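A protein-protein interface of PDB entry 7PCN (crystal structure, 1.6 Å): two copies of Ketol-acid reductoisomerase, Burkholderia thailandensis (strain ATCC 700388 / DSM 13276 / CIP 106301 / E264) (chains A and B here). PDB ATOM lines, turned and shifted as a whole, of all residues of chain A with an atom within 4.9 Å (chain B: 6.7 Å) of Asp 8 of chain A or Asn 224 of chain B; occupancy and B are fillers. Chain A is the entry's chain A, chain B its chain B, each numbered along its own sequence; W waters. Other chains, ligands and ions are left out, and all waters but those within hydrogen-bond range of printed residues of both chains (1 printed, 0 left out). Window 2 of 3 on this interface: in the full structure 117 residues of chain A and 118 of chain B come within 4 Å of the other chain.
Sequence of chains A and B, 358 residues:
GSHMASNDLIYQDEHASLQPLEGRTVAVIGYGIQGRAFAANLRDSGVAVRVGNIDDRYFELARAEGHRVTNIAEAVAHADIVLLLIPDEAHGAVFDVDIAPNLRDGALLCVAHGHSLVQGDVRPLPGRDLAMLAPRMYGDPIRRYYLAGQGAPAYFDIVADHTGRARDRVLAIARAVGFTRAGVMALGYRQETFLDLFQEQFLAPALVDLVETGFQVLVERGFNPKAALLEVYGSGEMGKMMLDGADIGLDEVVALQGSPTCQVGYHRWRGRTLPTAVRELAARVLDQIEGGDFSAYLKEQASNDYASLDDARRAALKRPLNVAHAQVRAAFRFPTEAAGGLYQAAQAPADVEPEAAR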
ATOM      1  N   ASP A   8      22.280 -10.582  12.894  1.00  0.00           N
ATOM      2  CA  ASP A   8      23.296 -11.597  12.500  1.00  0.00           C
ATOM      3  C   ASP A   8      24.089 -11.100  11.288  1.00  0.00           C
ATOM      4  O   ASP A   8      23.474 -10.488  10.390  1.00  0.00           O
ATOM      5  CB  ASP A   8      22.656 -12.950  12.207  1.00  0.00           C
ATOM      6  CG  ASP A   8      22.058 -13.578  13.447  1.00  0.00           C
ATOM      7  OD1 ASP A   8      22.761 -13.616  14.478  1.00  0.00           O
ATOM      8  OD2 ASP A   8      20.903 -14.019  13.367  1.00  0.00           O
ATOM      9  N   LEU A   9      25.394 -11.381  11.263  1.00  0.00           N
ATOM     10  CA  LEU A   9      26.296 -11.094  10.115  1.00  0.00           C
ATOM     11  C   LEU A   9      26.507 -12.387   9.340  1.00  0.00           C
ATOM     12  O   LEU A   9      27.194 -13.279   9.878  1.00  0.00           O
ATOM     13  CB  LEU A   9      27.653 -10.576  10.609  1.00  0.00           C
ATOM     14  CG  LEU A   9      27.623  -9.388  11.566  1.00  0.00           C
ATOM     15  CD1 LEU A   9      29.039  -8.946  11.900  1.00  0.00           C
ATOM     16  CD2 LEU A   9      26.830  -8.238  10.975  1.00  0.00           C
ATOM     17  N   ILE A  10      25.924 -12.488   8.144  1.00  0.00           N
ATOM     18  CA  ILE A  10      25.962 -13.724   7.318  1.00  0.00           C
ATOM     19  C   ILE A  10      26.567 -13.351   5.969  1.00  0.00           C
ATOM     20  O   ILE A  10      26.000 -12.504   5.263  1.00  0.00           O
ATOM     21  CB  ILE A  10      24.562 -14.360   7.209  1.00  0.00           C
ATOM     22  CG1 ILE A  10      24.011 -14.700   8.600  1.00  0.00           C
ATOM     23  CG2 ILE A  10      24.591 -15.581   6.296  1.00  0.00           C
ATOM     24  CD1 ILE A  10      22.545 -15.012   8.633  1.00  0.00           C
ATOM     25  N   MET A 185      28.359 -17.372   9.121  1.00  0.00           N
ATOM     26  CA  MET A 185      27.781 -16.457  10.123  1.00  0.00           C
ATOM     27  C   MET A 185      28.796 -16.194  11.237  1.00  0.00           C
ATOM     28  O   MET A 185      29.447 -17.143  11.684  1.00  0.00           O
ATOM     29  CB  MET A 185      26.503 -17.043  10.715  1.00  0.00           C
ATOM     30  CG  MET A 185      25.830 -16.114  11.673  1.00  0.00           C
ATOM     31  SD  MET A 185      24.144 -16.637  12.094  1.00  0.00           S
ATOM     32  CE  MET A 185      24.425 -18.021  13.193  1.00  0.00           C
ATOM     33  N   LEU A 187      29.875 -16.004  14.843  1.00  0.00           N
ATOM     34  CA  LEU A 187      29.478 -16.594  16.142  1.00  0.00           C
ATOM     35  C   LEU A 187      30.740 -16.723  16.995  1.00  0.00           C
ATOM     36  O   LEU A 187      31.730 -17.265  16.479  1.00  0.00           O
ATOM     37  CB  LEU A 187      28.818 -17.953  15.910  1.00  0.00           C
ATOM     38  CG  LEU A 187      28.050 -18.496  17.114  1.00  0.00           C
ATOM     39  CD1 LEU A 187      26.679 -17.851  17.225  1.00  0.00           C
ATOM     40  CD2 LEU A 187      27.904 -19.999  17.024  1.00  0.00           C
ATOM     41  N   GLN A 191      30.750 -19.787  22.299  1.00  0.00           N
ATOM     42  CA  GLN A 191      29.379 -20.247  21.965  1.00  0.00           C
ATOM     43  C   GLN A 191      29.455 -21.423  20.974  1.00  0.00           C
ATOM     44  O   GLN A 191      28.757 -22.422  21.198  1.00  0.00           O
ATOM     45  CB  GLN A 191      28.521 -19.127  21.388  1.00  0.00           C
ATOM     46  CG  GLN A 191      27.111 -19.626  21.129  1.00  0.00           C
ATOM     47  CD  GLN A 191      26.100 -18.615  20.674  1.00  0.00           C
ATOM     48  OE1 GLN A 191      25.008 -18.996  20.245  1.00  0.00           O
ATOM     49  NE2 GLN A 191      26.446 -17.339  20.769  1.00  0.00           N
ATOM     50  N   PHE B 215      16.451 -27.566  20.039  1.00  0.00           N
ATOM     51  CA  PHE B 215      16.324 -26.160  19.600  1.00  0.00           C
ATOM     52  C   PHE B 215      15.884 -25.299  20.794  1.00  0.00           C
ATOM     53  O   PHE B 215      16.532 -24.283  21.081  1.00  0.00           O
ATOM     54  CB  PHE B 215      15.347 -26.034  18.432  1.00  0.00           C
ATOM     55  CG  PHE B 215      14.995 -24.607  18.116  1.00  0.00           C
ATOM     56  CD1 PHE B 215      15.873 -23.804  17.401  1.00  0.00           C
ATOM     57  CD2 PHE B 215      13.796 -24.066  18.545  1.00  0.00           C
ATOM     58  CE1 PHE B 215      15.545 -22.489  17.111  1.00  0.00           C
ATOM     59  CE2 PHE B 215      13.471 -22.752  18.257  1.00  0.00           C
ATOM     60  CZ  PHE B 215      14.346 -21.967  17.539  1.00  0.00           C
ATOM     61  N   LEU B 218      18.409 -24.839  23.705  1.00  0.00           N
ATOM     62  CA  LEU B 218      19.547 -23.977  23.290  1.00  0.00           C
ATOM     63  C   LEU B 218      19.101 -22.510  23.283  1.00  0.00           C
ATOM     64  O   LEU B 218      19.834 -21.684  23.806  1.00  0.00           O
ATOM     65  CB  LEU B 218      20.049 -24.392  21.908  1.00  0.00           C
ATOM     66  CG  LEU B 218      20.892 -25.662  21.852  1.00  0.00           C
ATOM     67  CD1 LEU B 218      21.046 -26.099  20.410  1.00  0.00           C
ATOM     68  CD2 LEU B 218      22.258 -25.433  22.492  1.00  0.00           C
ATOM     69  N   VAL B 219      17.941 -22.202  22.702  1.00  0.00           N
ATOM     70  CA  VAL B 219      17.447 -20.798  22.592  1.00  0.00           C
ATOM     71  C   VAL B 219      17.205 -20.248  24.001  1.00  0.00           C
ATOM     72  O   VAL B 219      17.653 -19.096  24.294  1.00  0.00           O
ATOM     73  CB  VAL B 219      16.195 -20.724  21.701  1.00  0.00           C
ATOM     74  CG1 VAL B 219      15.480 -19.380  21.830  1.00  0.00           C
ATOM     75  CG2 VAL B 219      16.572 -21.015  20.253  1.00  0.00           C
ATOM     76  N   GLY B 222      20.317 -19.123  25.838  1.00  0.00           N
ATOM     77  CA  GLY B 222      20.928 -17.888  25.310  1.00  0.00           C
ATOM     78  C   GLY B 222      21.690 -18.087  24.014  1.00  0.00           C
ATOM     79  O   GLY B 222      22.410 -17.153  23.608  1.00  0.00           O
ATOM     80  N   PHE B 223      21.558 -19.241  23.370  1.00  0.00           N
ATOM     81  CA  PHE B 223      22.229 -19.528  22.078  1.00  0.00           C
ATOM     82  C   PHE B 223      21.520 -18.778  20.943  1.00  0.00           C
ATOM     83  O   PHE B 223      20.278 -18.610  20.970  1.00  0.00           O
ATOM     84  CB  PHE B 223      22.317 -21.036  21.830  1.00  0.00           C
ATOM     85  CG  PHE B 223      23.308 -21.708  22.741  1.00  0.00           C
ATOM     86  CD1 PHE B 223      22.939 -22.103  24.019  1.00  0.00           C
ATOM     87  CD2 PHE B 223      24.631 -21.862  22.356  1.00  0.00           C
ATOM     88  CE1 PHE B 223      23.862 -22.678  24.875  1.00  0.00           C
ATOM     89  CE2 PHE B 223      25.555 -22.429  23.222  1.00  0.00           C
ATOM     90  CZ  PHE B 223      25.170 -22.850  24.474  1.00  0.00           C
ATOM     91  N   ASN B 224      22.318 -18.338  19.972  1.00  0.00           N
ATOM     92  CA  ASN B 224      21.847 -17.735  18.702  1.00  0.00           C
ATOM     93  C   ASN B 224      20.773 -18.650  18.094  1.00  0.00           C
ATOM     94  O   ASN B 224      21.048 -19.822  17.821  1.00  0.00           O
ATOM     95  CB  ASN B 224      23.058 -17.496  17.805  1.00  0.00           C
ATOM     96  CG  ASN B 224      22.719 -16.853  16.482  1.00  0.00           C
ATOM     97  OD1 ASN B 224      21.965 -17.423  15.694  1.00  0.00           O
ATOM     98  ND2 ASN B 224      23.302 -15.689  16.224  1.00  0.00           N
ATOM     99  N   PRO B 225      19.500 -18.196  17.928  1.00  0.00           N
ATOM    100  CA  PRO B 225      18.447 -19.078  17.409  1.00  0.00           C
ATOM    101  C   PRO B 225      18.711 -19.659  16.007  1.00  0.00           C
ATOM    102  O   PRO B 225      18.351 -20.801  15.751  1.00  0.00           O
ATOM    103  CB  PRO B 225      17.180 -18.207  17.409  1.00  0.00           C
ATOM    104  CG  PRO B 225      17.455 -17.150  18.464  1.00  0.00           C
ATOM    105  CD  PRO B 225      18.959 -16.913  18.413  1.00  0.00           C
ATOM    106  N   LYS B 226      19.326 -18.890  15.112  1.00  0.00           N
ATOM    107  CA  LYS B 226      19.660 -19.409  13.761  1.00  0.00           C
ATOM    108  C   LYS B 226      20.669 -20.558  13.913  1.00  0.00           C
ATOM    109  O   LYS B 226      20.492 -21.608  13.249  1.00  0.00           O
ATOM    110  CB  LYS B 226      20.187 -18.301  12.845  1.00  0.00           C
ATOM    111  CG  LYS B 226      19.174 -17.276  12.369  1.00  0.00           C
ATOM    112  CD  LYS B 226      19.750 -16.401  11.274  1.00  0.00           C
ATOM    113  CE  LYS B 226      18.799 -15.348  10.750  1.00  0.00           C
ATOM    114  NZ  LYS B 226      18.615 -14.245  11.719  1.00  0.00           N
ATOM    115  N   ALA B 227      21.708 -20.375  14.732  1.00  0.00           N
ATOM    116  CA  ALA B 227      22.750 -21.408  14.958  1.00  0.00           C
ATOM    117  C   ALA B 227      22.107 -22.652  15.596  1.00  0.00           C
ATOM    118  O   ALA B 227      22.379 -23.779  15.140  1.00  0.00           O
ATOM    119  CB  ALA B 227      23.883 -20.848  15.794  1.00  0.00           C
ATOM    120  N   ALA B 228      21.242 -22.460  16.592  1.00  0.00           N
ATOM    121  CA  ALA B 228      20.530 -23.569  17.269  1.00  0.00           C
ATOM    122  C   ALA B 228      19.729 -24.366  16.223  1.00  0.00           C
ATOM    123  O   ALA B 228      19.838 -25.610  16.203  1.00  0.00           O
ATOM    124  CB  ALA B 228      19.665 -23.038  18.381  1.00  0.00           C
ATOM    125  N   LEU B 229      18.990 -23.683  15.352  1.00  0.00           N
ATOM    126  CA  LEU B 229      18.146 -24.329  14.307  1.00  0.00           C
ATOM    127  C   LEU B 229      19.068 -25.089  13.340  1.00  0.00           C
ATOM    128  O   LEU B 229      18.803 -26.278  13.036  1.00  0.00           O
ATOM    129  CB  LEU B 229      17.329 -23.243  13.593  1.00  0.00           C
ATOM    130  CG  LEU B 229      16.170 -23.684  12.682  1.00  0.00           C
ATOM    131  CD1 LEU B 229      16.632 -24.431  11.437  1.00  0.00           C
ATOM    132  CD2 LEU B 229      15.133 -24.492  13.436  1.00  0.00           C
HETATM  133  O   HOH W   1      19.847 -15.158  15.302  1.00  0.00           O
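Of chain B, only Asn 224 (2.8 Å) and Lys 226 (2.8 Å) come within 4 Å of Asp 8 of chain A. Asn 224 of chain B touches just these residues of chain A: Asp 8 (2.8 Å), Met 185 (3.6 Å), Leu 187 (3.7 Å) and Gln 191 (2.8 Å). Of the printed residues of chain A, Lys 226 of chain B touches Asp 8. Printed residues of chain A within 4 Å of Ala 227 of chain B: Met 185 (3.9 Å).
No position is printed for both chains.
The backbone NH (N) of Asn 224 of chain B sits at hydrogen-bond distance from the side-chain amide oxygen (OE1) of Gln 191 of chain A. The side-chain carboxylate (OD2) of Asp 8 of chain A lies within salt-bridge range of the side-chain amino group (NZ) of Lys 226 of chain B (2.8 Å). The side-chain carboxylate of Asp 8 of chain A lies within hydrogen-bond range of the side-chain amide nitrogen of Asn 224 of chain B, at 2.8 Å.
Among the printed residues, merely in contact across the chains: Gln 191 of chain A with Phe 223 of chain B (3.4 Å), Met 185 of chain A with Asn 224 of chain B (3.6 Å), Leu 187 of chain A with Asn 224 of chain B (3.7 Å) and Met 185 of chain A with Ala 227 of chain B (3.9 Å).
Of the 6 printed residues of chain A, 4 touch a printed residue of chain B. Hydrophobic or aromatic side chains of chain B within 4 Å of the printed part of chain A: Phe 223 and Ala 227. Among the printed residues, 7 pairs touch across the chains.
OD1 of Asn 224 of chain B is in hydrogen-bond range of N of Lys 226 of chain B (3.1 Å). O of Leu 218 of chain B sits at hydrogen-bond distance from N of Phe 223 of chain B (3.0 Å). OD1 of Asn 224 of chain B lies within hydrogen-bond range of N of Ala 227 of chain B, at 3.1 Å.
Water W1 lies within hydrogen-bond range of the side-chain carboxylate (OD2) of Asp 8 of chain A (2.5 Å) and the side-chain amide oxygen (OD1) of Asn 224 of chain B (3.1 Å).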
